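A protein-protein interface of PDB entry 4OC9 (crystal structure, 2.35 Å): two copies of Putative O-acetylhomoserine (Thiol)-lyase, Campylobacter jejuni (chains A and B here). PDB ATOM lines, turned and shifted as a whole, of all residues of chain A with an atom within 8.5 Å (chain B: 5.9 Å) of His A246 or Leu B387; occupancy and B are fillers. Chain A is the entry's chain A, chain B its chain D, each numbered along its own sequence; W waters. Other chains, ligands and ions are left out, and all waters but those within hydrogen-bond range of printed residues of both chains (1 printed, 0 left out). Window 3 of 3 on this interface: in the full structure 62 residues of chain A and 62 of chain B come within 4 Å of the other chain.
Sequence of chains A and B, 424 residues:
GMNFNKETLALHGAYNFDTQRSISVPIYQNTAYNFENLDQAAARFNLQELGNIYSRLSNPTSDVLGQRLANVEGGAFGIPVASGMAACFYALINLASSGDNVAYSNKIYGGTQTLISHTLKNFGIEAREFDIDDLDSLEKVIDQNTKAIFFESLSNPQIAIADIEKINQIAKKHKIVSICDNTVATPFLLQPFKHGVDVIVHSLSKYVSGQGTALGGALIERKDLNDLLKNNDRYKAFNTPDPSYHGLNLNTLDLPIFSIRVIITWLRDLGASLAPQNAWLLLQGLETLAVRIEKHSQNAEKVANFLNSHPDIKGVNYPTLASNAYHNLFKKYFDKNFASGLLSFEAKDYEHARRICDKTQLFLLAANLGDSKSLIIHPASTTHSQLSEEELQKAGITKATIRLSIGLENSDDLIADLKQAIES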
ATOM      1  N   PHE A  45      -7.495 -18.160  19.549  1.00  0.00           N
ATOM      2  CA  PHE A  45      -7.482 -19.270  18.602  1.00  0.00           C
ATOM      3  C   PHE A  45      -8.863 -19.910  18.431  1.00  0.00           C
ATOM      4  O   PHE A  45      -9.078 -20.620  17.474  1.00  0.00           O
ATOM      5  CB  PHE A  45      -6.441 -20.337  18.988  1.00  0.00           C
ATOM      6  CG  PHE A  45      -5.040 -19.954  18.679  1.00  0.00           C
ATOM      7  CD1 PHE A  45      -4.300 -19.188  19.541  1.00  0.00           C
ATOM      8  CD2 PHE A  45      -4.461 -20.380  17.502  1.00  0.00           C
ATOM      9  CE1 PHE A  45      -3.000 -18.837  19.220  1.00  0.00           C
ATOM     10  CE2 PHE A  45      -3.166 -20.051  17.181  1.00  0.00           C
ATOM     11  CZ  PHE A  45      -2.421 -19.291  18.051  1.00  0.00           C
ATOM     12  N   ASN A  46      -9.775 -19.668  19.369  1.00  0.00           N
ATOM     13  CA  ASN A  46     -11.149 -20.218  19.347  1.00  0.00           C
ATOM     14  C   ASN A  46     -12.206 -19.244  18.927  1.00  0.00           C
ATOM     15  O   ASN A  46     -13.392 -19.523  19.028  1.00  0.00           O
ATOM     16  CB  ASN A  46     -11.568 -20.611  20.760  1.00  0.00           C
ATOM     17  CG  ASN A  46     -10.723 -21.698  21.341  1.00  0.00           C
ATOM     18  OD1 ASN A  46     -10.089 -22.467  20.614  1.00  0.00           O
ATOM     19  ND2 ASN A  46     -10.732 -21.797  22.668  1.00  0.00           N
ATOM     20  N   LEU A  47     -11.784 -18.082  18.460  1.00  0.00           N
ATOM     21  CA  LEU A  47     -12.713 -17.033  18.041  1.00  0.00           C
ATOM     22  C   LEU A  47     -13.595 -16.504  19.184  1.00  0.00           C
ATOM     23  O   LEU A  47     -14.550 -15.782  18.931  1.00  0.00           O
ATOM     24  CB  LEU A  47     -13.563 -17.411  16.831  1.00  0.00           C
ATOM     25  CG  LEU A  47     -12.835 -17.684  15.520  1.00  0.00           C
ATOM     26  CD1 LEU A  47     -11.990 -18.949  15.583  1.00  0.00           C
ATOM     27  CD2 LEU A  47     -13.890 -17.805  14.434  1.00  0.00           C
ATOM     28  N   PRO A 241     -21.904 -26.774  10.651  1.00  0.00           N
ATOM     29  CA  PRO A 241     -20.762 -26.930  11.538  1.00  0.00           C
ATOM     30  C   PRO A 241     -19.520 -27.207  10.710  1.00  0.00           C
ATOM     31  O   PRO A 241     -19.555 -28.026   9.792  1.00  0.00           O
ATOM     32  CB  PRO A 241     -21.122 -28.149  12.379  1.00  0.00           C
ATOM     33  CG  PRO A 241     -22.609 -28.214  12.347  1.00  0.00           C
ATOM     34  CD  PRO A 241     -23.006 -27.700  10.994  1.00  0.00           C
ATOM     35  N   ASP A 242     -18.429 -26.518  11.024  1.00  0.00           N
ATOM     36  CA  ASP A 242     -17.192 -26.687  10.277  1.00  0.00           C
ATOM     37  C   ASP A 242     -16.186 -27.493  11.089  1.00  0.00           C
ATOM     38  O   ASP A 242     -15.831 -27.104  12.205  1.00  0.00           O
ATOM     39  CB  ASP A 242     -16.650 -25.308   9.893  1.00  0.00           C
ATOM     40  CG  ASP A 242     -15.451 -25.371   8.957  1.00  0.00           C
ATOM     41  OD1 ASP A 242     -14.699 -26.361   8.970  1.00  0.00           O
ATOM     42  OD2 ASP A 242     -15.266 -24.392   8.208  1.00  0.00           O
ATOM     43  N   PRO A 243     -15.723 -28.626  10.524  1.00  0.00           N
ATOM     44  CA  PRO A 243     -14.757 -29.474  11.229  1.00  0.00           C
ATOM     45  C   PRO A 243     -13.404 -28.794  11.459  1.00  0.00           C
ATOM     46  O   PRO A 243     -12.742 -29.108  12.440  1.00  0.00           O
ATOM     47  CB  PRO A 243     -14.619 -30.698  10.307  1.00  0.00           C
ATOM     48  CG  PRO A 243     -14.954 -30.188   8.957  1.00  0.00           C
ATOM     49  CD  PRO A 243     -15.993 -29.120   9.158  1.00  0.00           C
ATOM     50  N   SER A 244     -12.999 -27.883  10.575  1.00  0.00           N
ATOM     51  CA  SER A 244     -11.725 -27.199  10.768  1.00  0.00           C
ATOM     52  C   SER A 244     -11.771 -26.378  12.070  1.00  0.00           C
ATOM     53  O   SER A 244     -10.715 -26.074  12.627  1.00  0.00           O
ATOM     54  CB  SER A 244     -11.319 -26.310   9.570  1.00  0.00           C
ATOM     55  OG  SER A 244     -12.218 -25.228   9.365  1.00  0.00           O
ATOM     56  N   TYR A 245     -12.976 -26.002  12.522  1.00  0.00           N
ATOM     57  CA  TYR A 245     -13.162 -25.226  13.770  1.00  0.00           C
ATOM     58  C   TYR A 245     -14.021 -25.877  14.833  1.00  0.00           C
ATOM     59  O   TYR A 245     -14.833 -25.218  15.487  1.00  0.00           O
ATOM     60  CB  TYR A 245     -13.608 -23.785  13.523  1.00  0.00           C
ATOM     61  CG  TYR A 245     -12.455 -22.943  13.069  1.00  0.00           C
ATOM     62  CD1 TYR A 245     -11.639 -22.309  14.011  1.00  0.00           C
ATOM     63  CD2 TYR A 245     -12.137 -22.813  11.722  1.00  0.00           C
ATOM     64  CE1 TYR A 245     -10.553 -21.550  13.630  1.00  0.00           C
ATOM     65  CE2 TYR A 245     -11.048 -22.056  11.327  1.00  0.00           C
ATOM     66  CZ  TYR A 245     -10.261 -21.428  12.278  1.00  0.00           C
ATOM     67  OH  TYR A 245      -9.173 -20.683  11.876  1.00  0.00           O
ATOM     68  N   HIS A 246     -13.775 -27.158  15.047  1.00  0.00           N
ATOM     69  CA  HIS A 246     -14.513 -27.920  16.040  1.00  0.00           C
ATOM     70  C   HIS A 246     -16.008 -27.674  16.023  1.00  0.00           C
ATOM     71  O   HIS A 246     -16.598 -27.280  17.035  1.00  0.00           O
ATOM     72  CB  HIS A 246     -13.934 -27.685  17.427  1.00  0.00           C
ATOM     73  CG  HIS A 246     -12.545 -28.203  17.559  1.00  0.00           C
ATOM     74  ND1 HIS A 246     -12.278 -29.517  17.879  1.00  0.00           N
ATOM     75  CD2 HIS A 246     -11.345 -27.603  17.376  1.00  0.00           C
ATOM     76  CE1 HIS A 246     -10.970 -29.705  17.899  1.00  0.00           C
ATOM     77  NE2 HIS A 246     -10.381 -28.559  17.599  1.00  0.00           N
ATOM     78  N   GLY A 247     -16.603 -27.890  14.854  1.00  0.00           N
ATOM     79  CA  GLY A 247     -18.044 -27.731  14.667  1.00  0.00           C
ATOM     80  C   GLY A 247     -18.651 -26.340  14.627  1.00  0.00           C
ATOM     81  O   GLY A 247     -19.872 -26.209  14.507  1.00  0.00           O
ATOM     82  N   LEU A 248     -17.834 -25.303  14.757  1.00  0.00           N
ATOM     83  CA  LEU A 248     -18.356 -23.943  14.713  1.00  0.00           C
ATOM     84  C   LEU A 248     -19.226 -23.728  13.491  1.00  0.00           C
ATOM     85  O   LEU A 248     -18.866 -24.134  12.374  1.00  0.00           O
ATOM     86  CB  LEU A 248     -17.219 -22.930  14.636  1.00  0.00           C
ATOM     87  CG  LEU A 248     -17.660 -21.476  14.465  1.00  0.00           C
ATOM     88  CD1 LEU A 248     -18.496 -20.975  15.639  1.00  0.00           C
ATOM     89  CD2 LEU A 248     -16.439 -20.581  14.278  1.00  0.00           C
ATOM     90  N   ASN A 249     -20.375 -23.094  13.699  1.00  0.00           N
ATOM     91  CA  ASN A 249     -21.298 -22.793  12.595  1.00  0.00           C
ATOM     92  C   ASN A 249     -21.316 -21.276  12.497  1.00  0.00           C
ATOM     93  O   ASN A 249     -21.736 -20.583  13.428  1.00  0.00           O
ATOM     94  CB  ASN A 249     -22.684 -23.387  12.823  1.00  0.00           C
ATOM     95  CG  ASN A 249     -23.607 -23.182  11.632  1.00  0.00           C
ATOM     96  OD1 ASN A 249     -23.531 -22.175  10.931  1.00  0.00           O
ATOM     97  ND2 ASN A 249     -24.523 -24.128  11.427  1.00  0.00           N
ATOM     98  N   ARG A 268      -5.633 -17.769   6.508  1.00  0.00           N
ATOM     99  CA  ARG A 268      -4.949 -18.719   7.370  1.00  0.00           C
ATOM    100  C   ARG A 268      -4.357 -19.920   6.666  1.00  0.00           C
ATOM    101  O   ARG A 268      -3.221 -20.290   6.961  1.00  0.00           O
ATOM    102  CB  ARG A 268      -5.871 -19.205   8.494  1.00  0.00           C
ATOM    103  CG  ARG A 268      -5.145 -20.063   9.506  1.00  0.00           C
ATOM    104  CD  ARG A 268      -6.009 -20.359  10.707  1.00  0.00           C
ATOM    105  NE  ARG A 268      -5.217 -20.963  11.785  1.00  0.00           N
ATOM    106  CZ  ARG A 268      -5.688 -21.315  12.983  1.00  0.00           C
ATOM    107  NH1 ARG A 268      -6.963 -21.130  13.308  1.00  0.00           N
ATOM    108  NH2 ARG A 268      -4.871 -21.863  13.876  1.00  0.00           N
ATOM    109  N   GLY B 110       0.491 -27.705  12.136  1.00  0.00           N
ATOM    110  CA  GLY B 110      -0.963 -27.662  12.263  1.00  0.00           C
ATOM    111  C   GLY B 110      -1.673 -26.967  11.130  1.00  0.00           C
ATOM    112  O   GLY B 110      -2.694 -27.455  10.614  1.00  0.00           O
ATOM    113  N   GLN B 113      -1.581 -28.983   8.116  1.00  0.00           N
ATOM    114  CA  GLN B 113      -2.450 -30.142   8.284  1.00  0.00           C
ATOM    115  C   GLN B 113      -3.877 -29.772   7.935  1.00  0.00           C
ATOM    116  O   GLN B 113      -4.565 -30.527   7.247  1.00  0.00           O
ATOM    117  CB  GLN B 113      -2.289 -30.705   9.705  1.00  0.00           C
ATOM    118  CG  GLN B 113      -3.066 -31.961  10.004  1.00  0.00           C
ATOM    119  CD  GLN B 113      -2.602 -32.581  11.302  1.00  0.00           C
ATOM    120  OE1 GLN B 113      -1.630 -32.127  11.916  1.00  0.00           O
ATOM    121  NE2 GLN B 113      -3.274 -33.646  11.720  1.00  0.00           N
ATOM    122  N   THR B 114      -4.306 -28.616   8.412  1.00  0.00           N
ATOM    123  CA  THR B 114      -5.655 -28.098   8.129  1.00  0.00           C
ATOM    124  C   THR B 114      -5.799 -27.835   6.626  1.00  0.00           C
ATOM    125  O   THR B 114      -6.790 -28.208   6.010  1.00  0.00           O
ATOM    126  CB  THR B 114      -5.934 -26.827   8.913  1.00  0.00           C
ATOM    127  OG1 THR B 114      -5.907 -27.140  10.316  1.00  0.00           O
ATOM    128  CG2 THR B 114      -7.267 -26.290   8.577  1.00  0.00           C
ATOM    129  N   THR B 383      -1.760 -23.791  18.613  1.00  0.00           N
ATOM    130  CA  THR B 383      -1.275 -24.146  17.246  1.00  0.00           C
ATOM    131  C   THR B 383      -1.887 -25.406  16.648  1.00  0.00           C
ATOM    132  O   THR B 383      -2.005 -25.543  15.434  1.00  0.00           O
ATOM    133  CB  THR B 383       0.266 -24.307  17.198  1.00  0.00           C
ATOM    134  OG1 THR B 383       0.679 -25.385  18.062  1.00  0.00           O
ATOM    135  CG2 THR B 383       0.970 -22.994  17.598  1.00  0.00           C
ATOM    136  N   HIS B 384      -2.248 -26.339  17.513  1.00  0.00           N
ATOM    137  CA  HIS B 384      -2.861 -27.585  17.094  1.00  0.00           C
ATOM    138  C   HIS B 384      -4.237 -27.719  17.746  1.00  0.00           C
ATOM    139  O   HIS B 384      -4.761 -28.815  17.973  1.00  0.00           O
ATOM    140  CB  HIS B 384      -1.897 -28.730  17.367  1.00  0.00           C
ATOM    141  CG  HIS B 384      -0.691 -28.685  16.482  1.00  0.00           C
ATOM    142  ND1 HIS B 384       0.302 -27.740  16.620  1.00  0.00           N
ATOM    143  CD2 HIS B 384      -0.306 -29.493  15.469  1.00  0.00           C
ATOM    144  CE1 HIS B 384       1.233 -27.944  15.709  1.00  0.00           C
ATOM    145  NE2 HIS B 384       0.895 -29.012  15.007  1.00  0.00           N
ATOM    146  N   SER B 385      -4.827 -26.551  17.989  1.00  0.00           N
ATOM    147  CA  SER B 385      -6.152 -26.413  18.574  1.00  0.00           C
ATOM    148  C   SER B 385      -7.226 -26.995  17.636  1.00  0.00           C
ATOM    149  O   SER B 385      -8.245 -27.520  18.094  1.00  0.00           O
ATOM    150  CB  SER B 385      -6.449 -24.927  18.824  1.00  0.00           C
ATOM    151  OG  SER B 385      -7.748 -24.734  19.354  1.00  0.00           O
ATOM    152  N   GLN B 386      -6.998 -26.893  16.325  1.00  0.00           N
ATOM    153  CA  GLN B 386      -7.945 -27.401  15.328  1.00  0.00           C
ATOM    154  C   GLN B 386      -8.009 -28.934  15.246  1.00  0.00           C
ATOM    155  O   GLN B 386      -9.069 -29.482  14.960  1.00  0.00           O
ATOM    156  CB  GLN B 386      -7.641 -26.793  13.947  1.00  0.00           C
ATOM    157  CG  GLN B 386      -7.915 -25.294  13.843  1.00  0.00           C
ATOM    158  CD  GLN B 386      -7.425 -24.683  12.540  1.00  0.00           C
ATOM    159  OE1 GLN B 386      -6.281 -24.906  12.110  1.00  0.00           O
ATOM    160  NE2 GLN B 386      -8.267 -23.866  11.931  1.00  0.00           N
ATOM    161  N   LEU B 387      -6.893 -29.612  15.532  1.00  0.00           N
ATOM    162  CA  LEU B 387      -6.834 -31.085  15.474  1.00  0.00           C
ATOM    163  C   LEU B 387      -7.755 -31.804  16.472  1.00  0.00           C
ATOM    164  O   LEU B 387      -8.064 -31.273  17.539  1.00  0.00           O
ATOM    165  CB  LEU B 387      -5.390 -31.608  15.619  1.00  0.00           C
ATOM    166  CG  LEU B 387      -4.323 -31.381  14.530  1.00  0.00           C
ATOM    167  CD1 LEU B 387      -4.059 -29.923  14.156  1.00  0.00           C
ATOM    168  CD2 LEU B 387      -3.028 -32.052  14.971  1.00  0.00           C
ATOM    169  N   SER B 388      -8.194 -33.012  16.098  1.00  0.00           N
ATOM    170  CA  SER B 388      -9.082 -33.828  16.946  1.00  0.00           C
ATOM    171  C   SER B 388      -8.273 -34.341  18.131  1.00  0.00           C
ATOM    172  O   SER B 388      -7.050 -34.398  18.057  1.00  0.00           O
ATOM    173  CB  SER B 388      -9.700 -35.003  16.176  1.00  0.00           C
ATOM    174  OG  SER B 388      -8.711 -35.924  15.767  1.00  0.00           O
ATOM    175  N   GLU B 389      -8.973 -34.765  19.183  1.00  0.00           N
ATOM    176  CA  GLU B 389      -8.339 -35.243  20.395  1.00  0.00           C
ATOM    177  C   GLU B 389      -7.428 -36.453  20.055  1.00  0.00           C
ATOM    178  O   GLU B 389      -6.351 -36.607  20.652  1.00  0.00           O
ATOM    179  CB  GLU B 389      -9.422 -35.495  21.478  1.00  0.00           C
ATOM    180  CG  GLU B 389      -8.953 -35.573  22.938  1.00  0.00           C
ATOM    181  CD  GLU B 389      -8.079 -36.758  23.293  1.00  0.00           C
ATOM    182  OE1 GLU B 389      -8.024 -37.747  22.540  1.00  0.00           O
ATOM    183  OE2 GLU B 389      -7.461 -36.716  24.373  1.00  0.00           O
ATOM    184  N   GLU B 391      -6.099 -37.121  16.769  1.00  0.00           N
ATOM    185  CA  GLU B 391      -5.027 -36.684  15.848  1.00  0.00           C
ATOM    186  C   GLU B 391      -3.851 -36.147  16.656  1.00  0.00           C
ATOM    187  O   GLU B 391      -2.703 -36.234  16.224  1.00  0.00           O
ATOM    188  CB  GLU B 391      -5.497 -35.602  14.857  1.00  0.00           C
ATOM    189  CG  GLU B 391      -6.412 -36.073  13.745  1.00  0.00           C
ATOM    190  CD  GLU B 391      -6.914 -34.929  12.877  1.00  0.00           C
ATOM    191  OE1 GLU B 391      -7.163 -33.821  13.408  1.00  0.00           O
ATOM    192  OE2 GLU B 391      -7.137 -35.150  11.668  1.00  0.00           O
ATOM    193  N   LEU B 392      -4.155 -35.575  17.819  1.00  0.00           N
ATOM    194  CA  LEU B 392      -3.136 -35.033  18.704  1.00  0.00           C
ATOM    195  C   LEU B 392      -2.228 -36.100  19.188  1.00  0.00           C
ATOM    196  O   LEU B 392      -1.018 -35.906  19.243  1.00  0.00           O
ATOM    197  CB  LEU B 392      -3.755 -34.407  19.940  1.00  0.00           C
ATOM    198  CG  LEU B 392      -4.493 -33.078  19.854  1.00  0.00           C
ATOM    199  CD1 LEU B 392      -5.077 -32.771  21.221  1.00  0.00           C
ATOM    200  CD2 LEU B 392      -3.518 -31.995  19.425  1.00  0.00           C
ATOM    201  N   ALA B 395       0.133 -37.395  16.542  1.00  0.00           N
ATOM    202  CA  ALA B 395       1.229 -36.436  16.338  1.00  0.00           C
ATOM    203  C   ALA B 395       2.104 -36.377  17.595  1.00  0.00           C
ATOM    204  O   ALA B 395       3.183 -35.747  17.603  1.00  0.00           O
ATOM    205  CB  ALA B 395       0.682 -35.042  16.029  1.00  0.00           C
ATOM    206  N   ILE B 397       1.037 -35.221  21.000  1.00  0.00           N
ATOM    207  CA  ILE B 397       0.901 -34.003  21.806  1.00  0.00           C
ATOM    208  C   ILE B 397      -0.059 -34.293  22.957  1.00  0.00           C
ATOM    209  O   ILE B 397      -0.958 -35.069  22.791  1.00  0.00           O
ATOM    210  CB  ILE B 397       0.327 -32.839  20.994  1.00  0.00           C
ATOM    211  CG1 ILE B 397       1.237 -32.508  19.803  1.00  0.00           C
ATOM    212  CG2 ILE B 397       0.127 -31.609  21.891  1.00  0.00           C
ATOM    213  CD1 ILE B 397       0.670 -31.478  18.825  1.00  0.00           C
HETATM  214  O   HOH W   1      -8.454 -22.886   9.315  1.00  0.00           O
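The side-chain amide oxygen (OD1) of Asn A46 sits at hydrogen-bond distance from the side-chain hydroxyl (OG) of Ser B385, 3.5 Å away.
The side-chain amide nitrogen (NE2) of Gln B386 sits close to the backbone carbonyl oxygen (O) of Ser A244 (3.4 Å).
The side-chain hydroxyl of Tyr A245 lies close to the side-chain amide nitrogen of Gln B386 (3.3 Å).
NE2 of His A246 lies within hydrogen-bond range of O of Ser B385 (2.4 Å).
O of Gln B386 is in hydrogen-bond range of NE2 of His A246.
The guanidinium group (NH1) of Arg A268 lies close to the side-chain amide nitrogen (NE2) of Gln B386, 3.3 Å away.
The side-chain carboxylate of Asp A242 sits at hydrogen-bond distance from the side-chain hydroxyl of Ser A244.
NH1 of Arg A268 lies within hydrogen-bond range of OH of Tyr A245 (2.7 Å).
The side-chain amide oxygen of Gln B386 sits at hydrogen-bond distance from the side-chain hydroxyl of Thr B114 (2.9 Å).
Printed residues of chain A that touch a printed residue of chain B: Asn A46, Ser A244, Tyr A245, His A246 and Arg A268.
Hydrophobic or aromatic side chains of chain A within 4 Å of the printed part of chain B: Tyr A245 and His A246.
Among the printed residues, no Asp or Glu carboxylate lies within 4 Å of a Lys or Arg side-chain nitrogen of the other chain.
Printed residues of chain B within 4 Å of Tyr A245: Gln B386 (3.2 Å).
His A246 touches just these residues of chain B: Ser B385, Gln B386 and Leu B387.
Of the printed residues of chain B, Arg A268 touches Gln B386 (3.3 Å).
Leu B387 touches one residue of chain A.
No residue of chain A comes within 4 Å of Ser B388.
The nearest residue of chain B that does not touch His A246 is Ser B388 (4.6 Å).
The nearest residue of chain A that does not touch Leu B387 is Ser A244 (6.0 Å).
Among the printed residues, pairs that only touch across the chains: His A246 with Leu B387.
Water W1 lies within hydrogen-bond range of the side-chain amide nitrogen (NE2) of Gln B386 and the side-chain hydroxyl (OH) of Tyr A245.
No position is printed for both chains.
Of the 7 pairs that touch across the chains among the printed residues, none has its exchanged pair printed and touching as well.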
